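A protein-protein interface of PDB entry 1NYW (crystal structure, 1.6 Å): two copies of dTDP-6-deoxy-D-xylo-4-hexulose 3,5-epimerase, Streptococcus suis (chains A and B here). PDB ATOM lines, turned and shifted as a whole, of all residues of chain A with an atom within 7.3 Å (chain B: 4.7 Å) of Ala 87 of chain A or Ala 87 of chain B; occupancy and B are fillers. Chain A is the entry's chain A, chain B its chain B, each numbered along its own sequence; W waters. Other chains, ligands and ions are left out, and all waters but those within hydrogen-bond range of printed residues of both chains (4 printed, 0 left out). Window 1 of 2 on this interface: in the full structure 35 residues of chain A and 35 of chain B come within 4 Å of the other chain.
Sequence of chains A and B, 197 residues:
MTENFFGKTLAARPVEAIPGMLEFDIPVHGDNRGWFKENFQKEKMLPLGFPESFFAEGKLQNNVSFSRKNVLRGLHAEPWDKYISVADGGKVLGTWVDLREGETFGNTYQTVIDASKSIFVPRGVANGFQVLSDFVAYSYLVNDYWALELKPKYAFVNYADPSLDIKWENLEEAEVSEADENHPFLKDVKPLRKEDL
Hydrophobic or aromatic side chains of chain A within 4 Å of the printed part of chain B: Val 64, Phe 66, Ala 87 and Ala 137.
Hydrophobic or aromatic side chains of chain B within 4 Å of the printed part of chain A: Trp 35, Val 64, Ala 87 and Ala 137.
Among the printed residues, 10 pairs touch across the chains.
Val 64 of chain A touches Trp 35 of chain B, but with the chains exchanged Trp 35 of chain A does not touch Val 64 of chain B (4.04 Å).
Val 64 of chain A touches Ala 87 of chain B, and with the chains exchanged Ala 87 of chain A touches Val 64 of chain B.
Ala 87 of chain B touches its own counterpart, Ala 87 of chain A.
Ala 87 of chain A touches Ala 137 of chain B, and with the chains exchanged Ala 137 of chain A touches Ala 87 of chain B.
Positions printed for both chains: 35, 64, 85, 86, 87, 88, 137 and 139.
Water W3 lies within hydrogen-bond range of the side-chain hydroxyl of Ser 139 of chain B (2.6 Å) and the side-chain amide oxygen of Asn 62 of chain A (2.9 Å).
Water W2 lies within hydrogen-bond range of the side-chain carboxylate of Asp 88 of chain A (2.7 Å) and the side-chain carboxylate of Asp 88 of chain B (2.7 Å).
Water W1 lies within hydrogen-bond range of OG of Ser 139 of chain B (2.7 Å), OD1 of Asn 62 of chain A (2.8 Å) and OG of Ser 139 of chain A (2.9 Å).
Water W4 lies within hydrogen-bond range of OG of Ser 139 of chain A (2.7 Å) and OG of Ser 139 of chain B (2.9 Å).
Of chain B, only Val 64, Ala 87 and Ala 137 come within 4 Å of Ala 87 of chain A.
Ala 87 of chain B touches three residues of chain A.
Of the printed residues of chain B, Lys 37 of chain A touches Val 64 (2.9 Å).
Of the printed residues of chain B, Val 64 of chain A touches Trp 35 (3.7 Å) and Ala 87 (3.1 Å).
The nearest residue of chain A that does not touch Ala 87 of chain B is Phe 66 of chain A (4.6 Å).
The nearest printed residue of chain A that does not touch Val 64 of chain B is Trp 35 of chain A (4.04 Å).
The backbone carbonyl oxygen (O) of Ala 137 of chain A sits at hydrogen-bond distance from the backbone NH (N) of Ala 87 of chain A (2.8 Å).
The side-chain amino group (NZ) of Lys 37 of chain A sits at hydrogen-bond distance from the backbone carbonyl oxygen (O) of Val 86 of chain A (2.9 Å).
The backbone NH (N) of Ala 87 of chain B is in hydrogen-bond range of the backbone carbonyl oxygen (O) of Ala 137 of chain B (2.9 Å).
The backbone carbonyl oxygen (O) of Ser 65 of chain A lies within hydrogen-bond range of the backbone NH (N) of Tyr 138 of chain A (2.8 Å).
The backbone NH of Ala 137 of chain B lies within hydrogen-bond range of the side-chain carboxylate of Asp 88 of chain B (3.1 Å).
The side-chain amino group (NZ) of Lys 37 of chain A lies within hydrogen-bond range of the side-chain amide oxygen (OD1) of Asn 39 of chain A (2.9 Å).
Among the printed residues, pairs that only touch across the chains: Val 64 of chain A with Ala 87 of chain B (3.1 Å), Ser 65 of chain A with Trp 35 of chain B (3.2 Å), Ala 87 of chain A with Val 64 of chain B (3.2 Å), Ala 137 of chain A with Ala 87 of chain B (3.4 Å), Ala 87 of chain A with Ala 137 of chain B (3.4 Å), Val 64 of chain A with Trp 35 of chain B (3.7 Å), Ala 87 of chain A with Ala 87 of chain B (3.8 Å) and Phe 66 of chain A with Asp 88 of chain B (3.9 Å).
The backbone NH of Phe 66 of chain A sits at hydrogen-bond distance from the backbone carbonyl oxygen of Trp 35 of chain B, 3.0 Å away.
N of Lys 37 of chain A lies within hydrogen-bond range of O of Val 64 of chain B, 2.9 Å away.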
ATOM      1  N   TRP A  35       2.502 -15.173 -34.532  1.00  0.00           N
ATOM      2  CA  TRP A  35       1.924 -16.313 -33.812  1.00  0.00           C
ATOM      3  C   TRP A  35       0.395 -16.368 -33.872  1.00  0.00           C
ATOM      4  O   TRP A  35      -0.282 -15.460 -34.289  1.00  0.00           O
ATOM      5  CB  TRP A  35       2.453 -16.442 -32.344  1.00  0.00           C
ATOM      6  CG  TRP A  35       2.397 -15.256 -31.463  1.00  0.00           C
ATOM      7  CD1 TRP A  35       3.439 -14.463 -31.109  1.00  0.00           C
ATOM      8  CD2 TRP A  35       1.231 -14.714 -30.815  1.00  0.00           C
ATOM      9  NE1 TRP A  35       2.999 -13.463 -30.268  1.00  0.00           N
ATOM     10  CE2 TRP A  35       1.643 -13.591 -30.079  1.00  0.00           C
ATOM     11  CE3 TRP A  35      -0.138 -15.042 -30.811  1.00  0.00           C
ATOM     12  CZ2 TRP A  35       0.743 -12.807 -29.320  1.00  0.00           C
ATOM     13  CZ3 TRP A  35      -1.021 -14.259 -30.044  1.00  0.00           C
ATOM     14  CH2 TRP A  35      -0.570 -13.152 -29.331  1.00  0.00           C
ATOM     15  N   LYS A  37      -3.054 -18.116 -31.499  1.00  0.00           N
ATOM     16  CA  LYS A  37      -3.639 -18.960 -30.459  1.00  0.00           C
ATOM     17  C   LYS A  37      -5.153 -19.117 -30.570  1.00  0.00           C
ATOM     18  O   LYS A  37      -5.843 -18.207 -31.028  1.00  0.00           O
ATOM     19  CB  LYS A  37      -3.322 -18.421 -29.062  1.00  0.00           C
ATOM     20  CG  LYS A  37      -3.722 -16.945 -28.851  1.00  0.00           C
ATOM     21  CD  LYS A  37      -3.573 -16.536 -27.380  1.00  0.00           C
ATOM     22  CE  LYS A  37      -3.923 -15.091 -27.098  1.00  0.00           C
ATOM     23  NZ  LYS A  37      -4.131 -14.824 -25.673  1.00  0.00           N
ATOM     24  N   ASN A  39      -7.529 -18.479 -28.237  1.00  0.00           N
ATOM     25  CA  ASN A  39      -7.632 -17.784 -26.944  1.00  0.00           C
ATOM     26  C   ASN A  39      -8.696 -18.389 -25.999  1.00  0.00           C
ATOM     27  O   ASN A  39      -8.505 -18.554 -24.748  1.00  0.00           O
ATOM     28  CB  ASN A  39      -7.907 -16.301 -27.139  1.00  0.00           C
ATOM     29  CG  ASN A  39      -7.895 -15.574 -25.835  1.00  0.00           C
ATOM     30  OD1 ASN A  39      -6.873 -15.504 -25.156  1.00  0.00           O
ATOM     31  ND2 ASN A  39      -9.038 -15.017 -25.484  1.00  0.00           N
ATOM     32  N   ASN A  62     -17.421  -8.930 -25.656  1.00  0.00           N
ATOM     33  CA  ASN A  62     -15.958  -9.019 -25.711  1.00  0.00           C
ATOM     34  C   ASN A  62     -15.453  -7.553 -25.653  1.00  0.00           C
ATOM     35  O   ASN A  62     -15.793  -6.773 -26.529  1.00  0.00           O
ATOM     36  CB  ASN A  62     -15.517  -9.673 -27.047  1.00  0.00           C
ATOM     37  CG  ASN A  62     -13.981  -9.556 -27.326  1.00  0.00           C
ATOM     38  OD1 ASN A  62     -13.553  -9.524 -28.454  1.00  0.00           O
ATOM     39  ND2 ASN A  62     -13.142  -9.609 -26.258  1.00  0.00           N
ATOM     40  N   VAL A  64     -12.075  -4.905 -25.136  1.00  0.00           N
ATOM     41  CA  VAL A  64     -10.656  -4.796 -25.392  1.00  0.00           C
ATOM     42  C   VAL A  64     -10.183  -3.434 -24.885  1.00  0.00           C
ATOM     43  O   VAL A  64     -10.786  -2.442 -25.125  1.00  0.00           O
ATOM     44  CB  VAL A  64     -10.252  -5.006 -26.841  1.00  0.00           C
ATOM     45  CG1 VAL A  64      -8.769  -4.874 -27.030  1.00  0.00           C
ATOM     46  CG2 VAL A  64     -10.816  -6.361 -27.409  1.00  0.00           C
ATOM     47  N   SER A  65      -9.126  -3.426 -24.060  1.00  0.00           N
ATOM     48  CA  SER A  65      -8.458  -2.165 -23.701  1.00  0.00           C
ATOM     49  C   SER A  65      -7.026  -2.228 -24.204  1.00  0.00           C
ATOM     50  O   SER A  65      -6.381  -3.268 -24.324  1.00  0.00           O
ATOM     51  CB  SER A  65      -8.474  -1.847 -22.171  1.00  0.00           C
ATOM     52  OG  SER A  65      -7.892  -2.879 -21.435  1.00  0.00           O
ATOM     53  N   PHE A  66      -6.509  -1.054 -24.502  1.00  0.00           N
ATOM     54  CA  PHE A  66      -5.148  -0.907 -24.938  1.00  0.00           C
ATOM     55  C   PHE A  66      -4.528   0.085 -24.017  1.00  0.00           C
ATOM     56  O   PHE A  66      -5.049   1.158 -23.789  1.00  0.00           O
ATOM     57  CB  PHE A  66      -5.150  -0.426 -26.403  1.00  0.00           C
ATOM     58  CG  PHE A  66      -3.768  -0.430 -27.014  1.00  0.00           C
ATOM     59  CD1 PHE A  66      -3.083  -1.604 -27.206  1.00  0.00           C
ATOM     60  CD2 PHE A  66      -3.146   0.781 -27.325  1.00  0.00           C
ATOM     61  CE1 PHE A  66      -1.824  -1.601 -27.724  1.00  0.00           C
ATOM     62  CE2 PHE A  66      -1.896   0.801 -27.857  1.00  0.00           C
ATOM     63  CZ  PHE A  66      -1.231  -0.411 -28.064  1.00  0.00           C
ATOM     64  N   SER A  85      -7.477 -12.321 -21.014  1.00  0.00           N
ATOM     65  CA  SER A  85      -6.192 -12.737 -21.520  1.00  0.00           C
ATOM     66  C   SER A  85      -5.545 -11.500 -22.164  1.00  0.00           C
ATOM     67  O   SER A  85      -6.170 -10.440 -22.201  1.00  0.00           O
ATOM     68  CB  SER A  85      -6.330 -13.910 -22.486  1.00  0.00           C
ATOM     69  OG  SER A  85      -5.002 -14.300 -22.940  1.00  0.00           O
ATOM     70  N   VAL A  86      -4.333 -11.674 -22.676  1.00  0.00           N
ATOM     71  CA  VAL A  86      -3.651 -10.586 -23.410  1.00  0.00           C
ATOM     72  C   VAL A  86      -3.679 -10.984 -24.902  1.00  0.00           C
ATOM     73  O   VAL A  86      -3.398 -12.083 -25.285  1.00  0.00           O
ATOM     74  CB  VAL A  86      -2.216 -10.463 -22.867  1.00  0.00           C
ATOM     75  CG1 VAL A  86      -1.291  -9.715 -23.803  1.00  0.00           C
ATOM     76  CG2 VAL A  86      -2.229  -9.799 -21.512  1.00  0.00           C
ATOM     77  N   ALA A  87      -3.953 -10.010 -25.731  1.00  0.00           N
ATOM     78  CA  ALA A  87      -4.118 -10.263 -27.132  1.00  0.00           C
ATOM     79  C   ALA A  87      -2.902  -9.939 -28.033  1.00  0.00           C
ATOM     80  O   ALA A  87      -2.892 -10.307 -29.232  1.00  0.00           O
ATOM     81  CB  ALA A  87      -5.348  -9.448 -27.629  1.00  0.00           C
ATOM     82  N   ASP A  88      -1.891  -9.228 -27.522  1.00  0.00           N
ATOM     83  CA  ASP A  88      -0.706  -8.889 -28.322  1.00  0.00           C
ATOM     84  C   ASP A  88       0.566  -9.410 -27.606  1.00  0.00           C
ATOM     85  O   ASP A  88       0.447 -10.354 -26.821  1.00  0.00           O
ATOM     86  CB  ASP A  88      -0.703  -7.365 -28.603  1.00  0.00           C
ATOM     87  CG  ASP A  88      -0.418  -6.491 -27.378  1.00  0.00           C
ATOM     88  OD1 ASP A  88      -0.480  -7.012 -26.229  1.00  0.00           O
ATOM     89  OD2 ASP A  88      -0.143  -5.257 -27.470  1.00  0.00           O
ATOM     90  N   GLY A  89       1.733  -8.804 -27.864  1.00  0.00           N
ATOM     91  CA  GLY A  89       2.991  -9.219 -27.295  1.00  0.00           C
ATOM     92  C   GLY A  89       3.299  -8.680 -25.921  1.00  0.00           C
ATOM     93  O   GLY A  89       4.392  -8.940 -25.364  1.00  0.00           O
ATOM     94  N   GLY A  90       2.333  -8.012 -25.317  1.00  0.00           N
ATOM     95  CA  GLY A  90       2.479  -7.366 -24.014  1.00  0.00           C
ATOM     96  C   GLY A  90       2.321  -8.240 -22.781  1.00  0.00           C
ATOM     97  O   GLY A  90       2.096  -9.422 -22.872  1.00  0.00           O
ATOM     98  N   ASP A 114       0.578 -12.964 -19.890  1.00  0.00           N
ATOM     99  CA  ASP A 114       0.906 -12.638 -21.306  1.00  0.00           C
ATOM    100  C   ASP A 114      -0.066 -13.421 -22.192  1.00  0.00           C
ATOM    101  O   ASP A 114      -0.966 -14.125 -21.680  1.00  0.00           O
ATOM    102  CB  ASP A 114       2.403 -12.846 -21.615  1.00  0.00           C
ATOM    103  CG  ASP A 114       2.876 -14.287 -21.515  1.00  0.00           C
ATOM    104  OD1 ASP A 114       2.046 -15.245 -21.599  1.00  0.00           O
ATOM    105  OD2 ASP A 114       4.096 -14.553 -21.327  1.00  0.00           O
ATOM    106  N   ALA A 115       0.152 -13.398 -23.507  1.00  0.00           N
ATOM    107  CA  ALA A 115      -0.811 -14.101 -24.385  1.00  0.00           C
ATOM    108  C   ALA A 115      -0.930 -15.623 -24.156  1.00  0.00           C
ATOM    109  O   ALA A 115      -1.923 -16.241 -24.562  1.00  0.00           O
ATOM    110  CB  ALA A 115      -0.466 -13.881 -25.779  1.00  0.00           C
ATOM    111  N   VAL A 136       0.033  -2.866 -23.941  1.00  0.00           N
ATOM    112  CA  VAL A 136      -0.600  -4.188 -23.933  1.00  0.00           C
ATOM    113  C   VAL A 136      -2.055  -4.107 -24.404  1.00  0.00           C
ATOM    114  O   VAL A 136      -2.723  -3.112 -24.111  1.00  0.00           O
ATOM    115  CB  VAL A 136      -0.582  -4.764 -22.552  1.00  0.00           C
ATOM    116  CG1 VAL A 136      -1.487  -3.980 -21.567  1.00  0.00           C
ATOM    117  CG2 VAL A 136      -0.916  -6.263 -22.595  1.00  0.00           C
ATOM    118  N   ALA A 137      -2.555  -5.153 -25.100  1.00  0.00           N
ATOM    119  CA  ALA A 137      -3.910  -5.286 -25.520  1.00  0.00           C
ATOM    120  C   ALA A 137      -4.510  -6.344 -24.625  1.00  0.00           C
ATOM    121  O   ALA A 137      -3.974  -7.432 -24.583  1.00  0.00           O
ATOM    122  CB  ALA A 137      -3.953  -5.763 -26.930  1.00  0.00           C
ATOM    123  N   TYR A 138      -5.479  -5.923 -23.862  1.00  0.00           N
ATOM    124  CA  TYR A 138      -6.155  -6.790 -22.887  1.00  0.00           C
ATOM    125  C   TYR A 138      -7.552  -7.078 -23.446  1.00  0.00           C
ATOM    126  O   TYR A 138      -8.327  -6.136 -23.630  1.00  0.00           O
ATOM    127  CB  TYR A 138      -6.170  -6.060 -21.536  1.00  0.00           C
ATOM    128  CG  TYR A 138      -6.704  -6.683 -20.329  1.00  0.00           C
ATOM    129  CD1 TYR A 138      -5.834  -7.275 -19.409  1.00  0.00           C
ATOM    130  CD2 TYR A 138      -8.037  -6.648 -20.043  1.00  0.00           C
ATOM    131  CE1 TYR A 138      -6.302  -7.817 -18.236  1.00  0.00           C
ATOM    132  CE2 TYR A 138      -8.563  -7.221 -18.849  1.00  0.00           C
ATOM    133  CZ  TYR A 138      -7.658  -7.753 -17.962  1.00  0.00           C
ATOM    134  OH  TYR A 138      -8.068  -8.331 -16.743  1.00  0.00           O
ATOM    135  N   SER A 139      -7.875  -8.348 -23.620  1.00  0.00           N
ATOM    136  CA  SER A 139      -9.147  -8.733 -24.235  1.00  0.00           C
ATOM    137  C   SER A 139      -9.844  -9.705 -23.342  1.00  0.00           C
ATOM    138  O   SER A 139      -9.197 -10.633 -22.873  1.00  0.00           O
ATOM    139  CB  SER A 139      -8.915  -9.393 -25.616  1.00  0.00           C
ATOM    140  OG  SER A 139     -10.131  -9.860 -26.221  1.00  0.00           O
ATOM    141  N   TRP B  35      -7.038   3.271 -24.409  1.00  0.00           N
ATOM    142  CA  TRP B  35      -8.455   3.196 -24.820  1.00  0.00           C
ATOM    143  C   TRP B  35      -9.186   1.967 -24.426  1.00  0.00           C
ATOM    144  O   TRP B  35      -8.570   1.005 -24.011  1.00  0.00           O
ATOM    145  CB  TRP B  35      -8.556   3.460 -26.303  1.00  0.00           C
ATOM    146  CG  TRP B  35      -7.798   2.587 -27.262  1.00  0.00           C
ATOM    147  CD1 TRP B  35      -6.830   3.052 -28.092  1.00  0.00           C
ATOM    148  CD2 TRP B  35      -8.078   1.237 -27.720  1.00  0.00           C
ATOM    149  NE1 TRP B  35      -6.351   2.059 -28.895  1.00  0.00           N
ATOM    150  CE2 TRP B  35      -7.136   0.941 -28.725  1.00  0.00           C
ATOM    151  CE3 TRP B  35      -8.987   0.214 -27.334  1.00  0.00           C
ATOM    152  CZ2 TRP B  35      -7.008  -0.306 -29.291  1.00  0.00           C
ATOM    153  CZ3 TRP B  35      -8.841  -1.011 -27.938  1.00  0.00           C
ATOM    154  CH2 TRP B  35      -7.869  -1.236 -28.932  1.00  0.00           C
ATOM    155  N   VAL B  64      -6.700 -15.521 -31.863  1.00  0.00           N
ATOM    156  CA  VAL B  64      -5.921 -14.307 -31.990  1.00  0.00           C
ATOM    157  C   VAL B  64      -4.651 -14.615 -32.749  1.00  0.00           C
ATOM    158  O   VAL B  64      -3.988 -15.577 -32.453  1.00  0.00           O
ATOM    159  CB  VAL B  64      -5.611 -13.696 -30.650  1.00  0.00           C
ATOM    160  CG1 VAL B  64      -4.692 -12.451 -30.791  1.00  0.00           C
ATOM    161  CG2 VAL B  64      -6.833 -13.372 -29.850  1.00  0.00           C
ATOM    162  N   SER B  85     -11.808  -8.466 -35.959  1.00  0.00           N
ATOM    163  CA  SER B  85     -11.437  -7.130 -35.516  1.00  0.00           C
ATOM    164  C   SER B  85      -9.932  -7.038 -35.148  1.00  0.00           C
ATOM    165  O   SER B  85      -9.189  -8.050 -35.198  1.00  0.00           O
ATOM    166  CB  SER B  85     -12.271  -6.761 -34.301  1.00  0.00           C
ATOM    167  OG  SER B  85     -11.952  -5.549 -33.770  1.00  0.00           O
ATOM    168  N   VAL B  86      -9.495  -5.820 -34.939  1.00  0.00           N
ATOM    169  CA  VAL B  86      -8.109  -5.576 -34.463  1.00  0.00           C
ATOM    170  C   VAL B  86      -8.140  -5.236 -32.973  1.00  0.00           C
ATOM    171  O   VAL B  86      -8.967  -4.422 -32.543  1.00  0.00           O
ATOM    172  CB  VAL B  86      -7.451  -4.468 -35.323  1.00  0.00           C
ATOM    173  CG1 VAL B  86      -6.201  -4.026 -34.677  1.00  0.00           C
ATOM    174  CG2 VAL B  86      -7.171  -4.987 -36.729  1.00  0.00           C
ATOM    175  N   ALA B  87      -7.261  -5.869 -32.180  1.00  0.00           N
ATOM    176  CA  ALA B  87      -7.247  -5.714 -30.702  1.00  0.00           C
ATOM    177  C   ALA B  87      -6.199  -4.734 -30.112  1.00  0.00           C
ATOM    178  O   ALA B  87      -6.286  -4.376 -28.899  1.00  0.00           O
ATOM    179  CB  ALA B  87      -7.057  -7.105 -30.096  1.00  0.00           C
ATOM    180  N   ASP B  88      -5.240  -4.325 -30.941  1.00  0.00           N
ATOM    181  CA  ASP B  88      -4.180  -3.404 -30.574  1.00  0.00           C
ATOM    182  C   ASP B  88      -4.180  -2.137 -31.363  1.00  0.00           C
ATOM    183  O   ASP B  88      -5.222  -1.779 -31.959  1.00  0.00           O
ATOM    184  CB  ASP B  88      -2.790  -4.109 -30.490  1.00  0.00           C
ATOM    185  CG  ASP B  88      -2.207  -4.429 -31.857  1.00  0.00           C
ATOM    186  OD1 ASP B  88      -2.962  -4.320 -32.850  1.00  0.00           O
ATOM    187  OD2 ASP B  88      -1.062  -4.910 -32.020  1.00  0.00           O
ATOM    188  N   ALA B 137      -2.496  -7.179 -33.812  1.00  0.00           N
ATOM    189  CA  ALA B 137      -3.205  -8.238 -33.113  1.00  0.00           C
ATOM    190  C   ALA B 137      -4.580  -8.366 -33.746  1.00  0.00           C
ATOM    191  O   ALA B 137      -5.382  -7.462 -33.652  1.00  0.00           O
ATOM    192  CB  ALA B 137      -3.323  -7.914 -31.601  1.00  0.00           C
ATOM    193  N   SER B 139      -8.001 -10.336 -33.801  1.00  0.00           N
ATOM    194  CA  SER B 139      -8.850 -11.190 -32.906  1.00  0.00           C
ATOM    195  C   SER B 139     -10.167 -11.438 -33.560  1.00  0.00           C
ATOM    196  O   SER B 139     -10.868 -10.501 -33.923  1.00  0.00           O
ATOM    197  CB  SER B 139      -8.988 -10.462 -31.536  1.00  0.00           C
ATOM    198  OG  SER B 139      -9.718 -11.226 -30.613  1.00  0.00           O
HETATM  199  O   HOH W   1     -10.848  -9.396 -28.975  1.00  0.00           O
HETATM  200  O   HOH W   2       0.527  -4.383 -29.900  1.00  0.00           O
HETATM  201  O   HOH W   3     -12.333 -10.903 -30.687  1.00  0.00           O
HETATM  202  O   HOH W   4      -9.297 -11.864 -27.866  1.00  0.00           O
